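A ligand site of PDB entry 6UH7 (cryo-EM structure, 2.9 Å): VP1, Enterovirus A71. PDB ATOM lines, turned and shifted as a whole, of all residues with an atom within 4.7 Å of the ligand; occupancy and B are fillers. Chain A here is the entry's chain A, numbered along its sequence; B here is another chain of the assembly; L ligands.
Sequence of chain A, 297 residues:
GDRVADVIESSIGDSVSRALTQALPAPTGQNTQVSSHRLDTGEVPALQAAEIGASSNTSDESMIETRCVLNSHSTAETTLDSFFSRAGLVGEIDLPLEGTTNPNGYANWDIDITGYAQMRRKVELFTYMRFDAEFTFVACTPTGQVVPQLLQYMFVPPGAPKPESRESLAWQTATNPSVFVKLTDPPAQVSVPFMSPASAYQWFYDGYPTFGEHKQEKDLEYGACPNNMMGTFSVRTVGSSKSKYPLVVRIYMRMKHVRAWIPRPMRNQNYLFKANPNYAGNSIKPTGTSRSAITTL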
ATOM      1  N   ILE A 111     -15.734 -19.680   6.603  1.00  0.00           N
ATOM      2  CA  ILE A 111     -16.837 -20.429   7.176  1.00  0.00           C
ATOM      3  C   ILE A 111     -16.734 -21.880   6.699  1.00  0.00           C
ATOM      4  O   ILE A 111     -16.903 -22.171   5.522  1.00  0.00           O
ATOM      5  CB  ILE A 111     -18.188 -19.823   6.807  1.00  0.00           C
ATOM      6  CG1 ILE A 111     -18.372 -18.465   7.471  1.00  0.00           C
ATOM      7  CG2 ILE A 111     -19.307 -20.753   7.221  1.00  0.00           C
ATOM      8  CD1 ILE A 111     -19.227 -17.559   6.700  1.00  0.00           C
ATOM      9  N   ASP A 112     -16.454 -22.772   7.642  1.00  0.00           N
ATOM     10  CA  ASP A 112     -16.623 -24.199   7.435  1.00  0.00           C
ATOM     11  C   ASP A 112     -16.867 -24.849   8.772  1.00  0.00           C
ATOM     12  O   ASP A 112     -16.116 -24.648   9.726  1.00  0.00           O
ATOM     13  CB  ASP A 112     -15.421 -24.816   6.705  1.00  0.00           C
ATOM     14  CG  ASP A 112     -14.105 -24.511   7.376  1.00  0.00           C
ATOM     15  OD1 ASP A 112     -14.085 -23.749   8.354  1.00  0.00           O
ATOM     16  OD2 ASP A 112     -13.085 -25.041   6.893  1.00  0.00           O
ATOM     17  N   ILE A 113     -17.940 -25.632   8.839  1.00  0.00           N
ATOM     18  CA  ILE A 113     -18.362 -26.268  10.067  1.00  0.00           C
ATOM     19  C   ILE A 113     -17.749 -27.654  10.227  1.00  0.00           C
ATOM     20  O   ILE A 113     -18.273 -28.488  10.967  1.00  0.00           O
ATOM     21  CB  ILE A 113     -19.899 -26.309  10.168  1.00  0.00           C
ATOM     22  CG1 ILE A 113     -20.507 -27.315   9.181  1.00  0.00           C
ATOM     23  CG2 ILE A 113     -20.443 -24.934   9.852  1.00  0.00           C
ATOM     24  CD1 ILE A 113     -22.011 -27.311   9.168  1.00  0.00           C
ATOM     25  N   THR A 114     -16.648 -27.928   9.531  1.00  0.00           N
ATOM     26  CA  THR A 114     -15.993 -29.225   9.506  1.00  0.00           C
ATOM     27  C   THR A 114     -14.724 -29.245  10.362  1.00  0.00           C
ATOM     28  O   THR A 114     -13.859 -30.103  10.169  1.00  0.00           O
ATOM     29  CB  THR A 114     -15.669 -29.623   8.078  1.00  0.00           C
ATOM     30  OG1 THR A 114     -14.892 -28.585   7.461  1.00  0.00           O
ATOM     31  CG2 THR A 114     -16.929 -29.837   7.286  1.00  0.00           C
ATOM     32  N   PHE A 135     -27.000 -18.808  13.966  1.00  0.00           N
ATOM     33  CA  PHE A 135     -25.665 -18.702  14.531  1.00  0.00           C
ATOM     34  C   PHE A 135     -25.713 -17.871  15.801  1.00  0.00           C
ATOM     35  O   PHE A 135     -26.505 -16.931  15.904  1.00  0.00           O
ATOM     36  CB  PHE A 135     -24.698 -18.084  13.544  1.00  0.00           C
ATOM     37  CG  PHE A 135     -24.229 -19.023  12.491  1.00  0.00           C
ATOM     38  CD1 PHE A 135     -24.969 -19.221  11.363  1.00  0.00           C
ATOM     39  CD2 PHE A 135     -23.044 -19.703  12.637  1.00  0.00           C
ATOM     40  CE1 PHE A 135     -24.554 -20.077  10.407  1.00  0.00           C
ATOM     41  CE2 PHE A 135     -22.620 -20.562  11.663  1.00  0.00           C
ATOM     42  CZ  PHE A 135     -23.373 -20.744  10.548  1.00  0.00           C
ATOM     43  N   PHE A 137     -22.967 -16.225  18.906  1.00  0.00           N
ATOM     44  CA  PHE A 137     -21.572 -15.870  19.160  1.00  0.00           C
ATOM     45  C   PHE A 137     -21.400 -15.583  20.641  1.00  0.00           C
ATOM     46  O   PHE A 137     -21.935 -14.604  21.152  1.00  0.00           O
ATOM     47  CB  PHE A 137     -21.152 -14.676  18.315  1.00  0.00           C
ATOM     48  CG  PHE A 137     -21.555 -14.772  16.873  1.00  0.00           C
ATOM     49  CD1 PHE A 137     -22.806 -14.357  16.458  1.00  0.00           C
ATOM     50  CD2 PHE A 137     -20.700 -15.291  15.940  1.00  0.00           C
ATOM     51  CE1 PHE A 137     -23.170 -14.465  15.159  1.00  0.00           C
ATOM     52  CE2 PHE A 137     -21.072 -15.395  14.637  1.00  0.00           C
ATOM     53  CZ  PHE A 137     -22.311 -14.986  14.240  1.00  0.00           C
ATOM     54  N   TYR A 153     -19.217  -7.858  14.182  1.00  0.00           N
ATOM     55  CA  TYR A 153     -19.243  -9.138  13.472  1.00  0.00           C
ATOM     56  C   TYR A 153     -19.761  -8.907  12.058  1.00  0.00           C
ATOM     57  O   TYR A 153     -20.978  -8.818  11.855  1.00  0.00           O
ATOM     58  CB  TYR A 153     -20.120 -10.150  14.205  1.00  0.00           C
ATOM     59  CG  TYR A 153     -19.740 -10.519  15.607  1.00  0.00           C
ATOM     60  CD1 TYR A 153     -18.427 -10.420  16.051  1.00  0.00           C
ATOM     61  CD2 TYR A 153     -20.689 -10.977  16.489  1.00  0.00           C
ATOM     62  CE1 TYR A 153     -18.107 -10.770  17.332  1.00  0.00           C
ATOM     63  CE2 TYR A 153     -20.364 -11.328  17.761  1.00  0.00           C
ATOM     64  CZ  TYR A 153     -19.076 -11.219  18.191  1.00  0.00           C
ATOM     65  OH  TYR A 153     -18.772 -11.573  19.476  1.00  0.00           O
ATOM     66  N   PHE A 155     -20.281 -10.117   8.170  1.00  0.00           N
ATOM     67  CA  PHE A 155     -20.361 -11.189   7.190  1.00  0.00           C
ATOM     68  C   PHE A 155     -19.803 -10.681   5.879  1.00  0.00           C
ATOM     69  O   PHE A 155     -20.316  -9.709   5.316  1.00  0.00           O
ATOM     70  CB  PHE A 155     -21.807 -11.657   7.030  1.00  0.00           C
ATOM     71  CG  PHE A 155     -22.017 -12.716   5.985  1.00  0.00           C
ATOM     72  CD1 PHE A 155     -21.058 -13.674   5.696  1.00  0.00           C
ATOM     73  CD2 PHE A 155     -23.205 -12.770   5.303  1.00  0.00           C
ATOM     74  CE1 PHE A 155     -21.289 -14.620   4.736  1.00  0.00           C
ATOM     75  CE2 PHE A 155     -23.436 -13.716   4.342  1.00  0.00           C
ATOM     76  CZ  PHE A 155     -22.482 -14.639   4.068  1.00  0.00           C
ATOM     77  N   PRO A 177     -23.869  -7.383   5.755  1.00  0.00           N
ATOM     78  CA  PRO A 177     -24.532  -7.371   7.070  1.00  0.00           C
ATOM     79  C   PRO A 177     -23.528  -7.424   8.207  1.00  0.00           C
ATOM     80  O   PRO A 177     -22.455  -8.013   8.094  1.00  0.00           O
ATOM     81  CB  PRO A 177     -25.423  -8.615   7.038  1.00  0.00           C
ATOM     82  CG  PRO A 177     -24.995  -9.406   5.954  1.00  0.00           C
ATOM     83  CD  PRO A 177     -24.054  -8.674   5.082  1.00  0.00           C
ATOM     84  N   SER A 178     -23.895  -6.778   9.308  1.00  0.00           N
ATOM     85  CA  SER A 178     -23.023  -6.657  10.467  1.00  0.00           C
ATOM     86  C   SER A 178     -23.848  -6.675  11.743  1.00  0.00           C
ATOM     87  O   SER A 178     -25.055  -6.446  11.724  1.00  0.00           O
ATOM     88  CB  SER A 178     -22.188  -5.386  10.401  1.00  0.00           C
ATOM     89  OG  SER A 178     -21.250  -5.342  11.446  1.00  0.00           O
ATOM     90  N   VAL A 179     -23.167  -6.960  12.839  1.00  0.00           N
ATOM     91  CA  VAL A 179     -23.752  -6.971  14.173  1.00  0.00           C
ATOM     92  C   VAL A 179     -22.736  -6.337  15.120  1.00  0.00           C
ATOM     93  O   VAL A 179     -21.588  -6.792  15.179  1.00  0.00           O
ATOM     94  CB  VAL A 179     -24.128  -8.384  14.648  1.00  0.00           C
ATOM     95  CG1 VAL A 179     -24.531  -8.377  16.087  1.00  0.00           C
ATOM     96  CG2 VAL A 179     -25.267  -8.951  13.844  1.00  0.00           C
ATOM     97  N   VAL A 190     -28.362 -14.502  15.280  1.00  0.00           N
ATOM     98  CA  VAL A 190     -28.940 -14.132  13.996  1.00  0.00           C
ATOM     99  C   VAL A 190     -29.341 -15.396  13.250  1.00  0.00           C
ATOM    100  O   VAL A 190     -28.709 -16.443  13.400  1.00  0.00           O
ATOM    101  CB  VAL A 190     -27.966 -13.286  13.156  1.00  0.00           C
ATOM    102  CG1 VAL A 190     -27.634 -12.014  13.879  1.00  0.00           C
ATOM    103  CG2 VAL A 190     -26.686 -14.040  12.866  1.00  0.00           C
ATOM    104  N   VAL A 192     -29.972 -17.227   9.517  1.00  0.00           N
ATOM    105  CA  VAL A 192     -29.339 -17.194   8.203  1.00  0.00           C
ATOM    106  C   VAL A 192     -30.156 -18.073   7.276  1.00  0.00           C
ATOM    107  O   VAL A 192     -30.715 -19.074   7.723  1.00  0.00           O
ATOM    108  CB  VAL A 192     -27.884 -17.668   8.265  1.00  0.00           C
ATOM    109  CG1 VAL A 192     -27.193 -17.410   6.978  1.00  0.00           C
ATOM    110  CG2 VAL A 192     -27.204 -16.957   9.376  1.00  0.00           C
ATOM    111  N   MET A 195     -28.195 -20.307   1.374  1.00  0.00           N
ATOM    112  CA  MET A 195     -27.499 -19.335   0.539  1.00  0.00           C
ATOM    113  C   MET A 195     -26.618 -19.978  -0.519  1.00  0.00           C
ATOM    114  O   MET A 195     -25.644 -19.365  -0.965  1.00  0.00           O
ATOM    115  CB  MET A 195     -26.670 -18.405   1.418  1.00  0.00           C
ATOM    116  CG  MET A 195     -27.453 -17.491   2.290  1.00  0.00           C
ATOM    117  SD  MET A 195     -26.464 -16.162   2.927  1.00  0.00           S
ATOM    118  CE  MET A 195     -25.300 -17.116   3.854  1.00  0.00           C
ATOM    119  N   TYR A 201     -26.490 -27.834   0.138  1.00  0.00           N
ATOM    120  CA  TYR A 201     -25.089 -27.993   0.463  1.00  0.00           C
ATOM    121  C   TYR A 201     -24.693 -29.447   0.250  1.00  0.00           C
ATOM    122  O   TYR A 201     -25.536 -30.328   0.128  1.00  0.00           O
ATOM    123  CB  TYR A 201     -24.818 -27.572   1.914  1.00  0.00           C
ATOM    124  CG  TYR A 201     -25.167 -26.130   2.208  1.00  0.00           C
ATOM    125  CD1 TYR A 201     -24.376 -25.094   1.744  1.00  0.00           C
ATOM    126  CD2 TYR A 201     -26.279 -25.812   2.960  1.00  0.00           C
ATOM    127  CE1 TYR A 201     -24.691 -23.796   2.019  1.00  0.00           C
ATOM    128  CE2 TYR A 201     -26.606 -24.519   3.230  1.00  0.00           C
ATOM    129  CZ  TYR A 201     -25.802 -23.510   2.765  1.00  0.00           C
ATOM    130  OH  TYR A 201     -26.109 -22.203   3.032  1.00  0.00           O
ATOM    131  N   GLN A 202     -23.390 -29.690   0.193  1.00  0.00           N
ATOM    132  CA  GLN A 202     -22.895 -31.046   0.034  1.00  0.00           C
ATOM    133  C   GLN A 202     -21.567 -31.192   0.747  1.00  0.00           C
ATOM    134  O   GLN A 202     -20.614 -30.479   0.443  1.00  0.00           O
ATOM    135  CB  GLN A 202     -22.779 -31.442  -1.437  1.00  0.00           C
ATOM    136  CG  GLN A 202     -21.931 -30.585  -2.306  1.00  0.00           C
ATOM    137  CD  GLN A 202     -22.189 -30.882  -3.771  1.00  0.00           C
ATOM    138  OE1 GLN A 202     -22.566 -29.989  -4.536  1.00  0.00           O
ATOM    139  NE2 GLN A 202     -22.012 -32.129  -4.154  1.00  0.00           N
ATOM    140  N   TRP A 203     -21.523 -32.128   1.685  1.00  0.00           N
ATOM    141  CA  TRP A 203     -20.362 -32.329   2.527  1.00  0.00           C
ATOM    142  C   TRP A 203     -19.306 -33.157   1.828  1.00  0.00           C
ATOM    143  O   TRP A 203     -18.137 -33.116   2.223  1.00  0.00           O
ATOM    144  CB  TRP A 203     -20.786 -32.991   3.848  1.00  0.00           C
ATOM    145  CG  TRP A 203     -22.037 -32.400   4.402  1.00  0.00           C
ATOM    146  CD1 TRP A 203     -23.250 -32.996   4.473  1.00  0.00           C
ATOM    147  CD2 TRP A 203     -22.201 -31.088   4.926  1.00  0.00           C
ATOM    148  NE1 TRP A 203     -24.162 -32.145   5.014  1.00  0.00           N
ATOM    149  CE2 TRP A 203     -23.543 -30.951   5.305  1.00  0.00           C
ATOM    150  CE3 TRP A 203     -21.341 -30.001   5.114  1.00  0.00           C
ATOM    151  CZ2 TRP A 203     -24.043 -29.795   5.872  1.00  0.00           C
ATOM    152  CZ3 TRP A 203     -21.840 -28.855   5.672  1.00  0.00           C
ATOM    153  CH2 TRP A 203     -23.180 -28.761   6.035  1.00  0.00           C
ATOM    154  N   ASN A 228     -20.330 -24.541  -1.388  1.00  0.00           N
ATOM    155  CA  ASN A 228     -20.295 -24.585   0.056  1.00  0.00           C
ATOM    156  C   ASN A 228     -19.408 -23.504   0.660  1.00  0.00           C
ATOM    157  O   ASN A 228     -19.513 -23.253   1.858  1.00  0.00           O
ATOM    158  CB  ASN A 228     -19.806 -25.955   0.524  1.00  0.00           C
ATOM    159  CG  ASN A 228     -20.689 -27.074   0.039  1.00  0.00           C
ATOM    160  OD1 ASN A 228     -21.888 -26.895  -0.169  1.00  0.00           O
ATOM    161  ND2 ASN A 228     -20.105 -28.238  -0.151  1.00  0.00           N
ATOM    162  N   MET A 230     -19.346 -20.365   1.582  1.00  0.00           N
ATOM    163  CA  MET A 230     -20.346 -19.332   1.784  1.00  0.00           C
ATOM    164  C   MET A 230     -19.754 -17.979   2.138  1.00  0.00           C
ATOM    165  O   MET A 230     -20.507 -17.014   2.301  1.00  0.00           O
ATOM    166  CB  MET A 230     -21.324 -19.755   2.881  1.00  0.00           C
ATOM    167  CG  MET A 230     -22.384 -20.727   2.413  1.00  0.00           C
ATOM    168  SD  MET A 230     -23.570 -20.015   1.289  1.00  0.00           S
ATOM    169  CE  MET A 230     -23.042 -20.752  -0.247  1.00  0.00           C
ATOM    170  N   PHE A 233     -16.321 -14.973   7.801  1.00  0.00           N
ATOM    171  CA  PHE A 233     -16.724 -14.274   9.011  1.00  0.00           C
ATOM    172  C   PHE A 233     -15.563 -13.422   9.512  1.00  0.00           C
ATOM    173  O   PHE A 233     -14.453 -13.930   9.662  1.00  0.00           O
ATOM    174  CB  PHE A 233     -17.142 -15.253  10.092  1.00  0.00           C
ATOM    175  CG  PHE A 233     -17.468 -14.612  11.404  1.00  0.00           C
ATOM    176  CD1 PHE A 233     -18.681 -13.999  11.592  1.00  0.00           C
ATOM    177  CD2 PHE A 233     -16.561 -14.619  12.443  1.00  0.00           C
ATOM    178  CE1 PHE A 233     -18.978 -13.419  12.781  1.00  0.00           C
ATOM    179  CE2 PHE A 233     -16.858 -14.039  13.632  1.00  0.00           C
ATOM    180  CZ  PHE A 233     -18.067 -13.439  13.802  1.00  0.00           C
ATOM    181  N   ALA A 275     -12.506 -30.553   5.625  1.00  0.00           N
ATOM    182  CA  ALA A 275     -12.962 -30.858   4.269  1.00  0.00           C
ATOM    183  C   ALA A 275     -11.968 -31.780   3.565  1.00  0.00           C
ATOM    184  O   ALA A 275     -11.513 -31.509   2.454  1.00  0.00           O
ATOM    185  CB  ALA A 275     -13.178 -29.577   3.476  1.00  0.00           C
ATOM    186  N   ILE B  24     -30.510 -11.665   8.715  1.00  0.00           N
ATOM    187  CA  ILE B  24     -29.444 -10.806   8.208  1.00  0.00           C
ATOM    188  C   ILE B  24     -29.692 -10.318   6.794  1.00  0.00           C
ATOM    189  O   ILE B  24     -29.207  -9.236   6.434  1.00  0.00           O
ATOM    190  CB  ILE B  24     -28.069 -11.506   8.256  1.00  0.00           C
ATOM    191  CG1 ILE B  24     -28.096 -12.885   7.606  1.00  0.00           C
ATOM    192  CG2 ILE B  24     -27.630 -11.650   9.663  1.00  0.00           C
ATOM    193  CD1 ILE B  24     -26.797 -13.323   7.085  1.00  0.00           C
HETATM  194  C1  LIG L   1     -17.137 -26.745   3.587  1.00  0.00           C
HETATM  195  O1  LIG L   1     -16.706 -28.069   3.818  1.00  0.00           O
HETATM  196  C2  LIG L   1     -18.647 -26.665   3.402  1.00  0.00           C
HETATM  197  N1  LIG L   1     -19.158 -27.772   2.579  1.00  0.00           N
HETATM  198  C3  LIG L   1     -19.371 -26.554   4.751  1.00  0.00           C
HETATM  199  O2  LIG L   1     -18.577 -25.839   5.680  1.00  0.00           O
HETATM  200  C4  LIG L   1     -20.711 -25.898   4.625  1.00  0.00           C
HETATM  201  C5  LIG L   1     -21.111 -24.875   5.328  1.00  0.00           C
HETATM  202  C6  LIG L   1     -22.500 -24.312   5.328  1.00  0.00           C
HETATM  203  C7  LIG L   1     -22.667 -23.146   6.254  1.00  0.00           C
HETATM  204  C8  LIG L   1     -23.802 -22.217   5.882  1.00  0.00           C
HETATM  205  C9  LIG L   1     -23.933 -21.011   6.774  1.00  0.00           C
HETATM  206  C10 LIG L   1     -23.045 -19.846   6.415  1.00  0.00           C
HETATM  207  C11 LIG L   1     -23.617 -18.488   6.760  1.00  0.00           C
HETATM  208  C12 LIG L   1     -22.699 -17.613   7.567  1.00  0.00           C
HETATM  209  C13 LIG L   1     -23.385 -16.813   8.638  1.00  0.00           C
HETATM  210  C14 LIG L   1     -22.622 -15.600   9.106  1.00  0.00           C
HETATM  211  C15 LIG L   1     -23.492 -14.472   9.613  1.00  0.00           C
HETATM  212  C16 LIG L   1     -22.771 -13.418  10.410  1.00  0.00           C
HETATM  213  C17 LIG L   1     -23.430 -12.061  10.356  1.00  0.00           C
HETATM  214  C18 LIG L   1     -23.042 -11.121  11.471  1.00  0.00           C
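Residues that only touch the ligand: Asp 112, Tyr 153, Trp 203, Ile 111, Met 195, Tyr 201, Phe 155, Val 192, Gln 202, Phe 135, Ala 275, Thr 114, Val 179 and Met 230.
Hydrophobic or aromatic side chains that line the ligand: Ile 111, Phe 135, Phe 155, Val 179, Val 192, Met 195, Tyr 201, Trp 203, Met 230 and Ala 275.
Within 4 Å of the ligand: Ile 111, Asp 112, Ile 113, Thr 114, Phe 135, Tyr 153, Phe 155, Val 179, Val 192, Met 195, Tyr 201, Gln 202, Trp 203, Asn 228, Met 230 and Ala 275.
Along chain A the residues within 4 Å of the ligand span positions 111 to 275.
O2 of the ligand sits at hydrogen-bond distance from N of Ile 113, at 3.2 Å.
ND2 of Asn 228 lies close to N1 of the ligand (2.9 Å).
The backbone NH (N) of Met 195 is in hydrogen-bond range of the side-chain hydroxyl (OH) of Tyr 201, 3.3 Å away.
The side-chain hydroxyl (OH) of Tyr 201 is in hydrogen-bond range of the side-chain sulfur (SD) of Met 230.
O of Val 190 lies within hydrogen-bond range of N of Phe 135, at 3.0 Å.
The backbone NH of Tyr 153 sits at hydrogen-bond distance from the backbone carbonyl oxygen of Val 179.
The backbone NH (N) of Phe 155 is in hydrogen-bond range of the backbone carbonyl oxygen (O) of Pro 177.
OD1 of Asn 228 is in hydrogen-bond range of N of Gln 202, at 3.2 Å.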
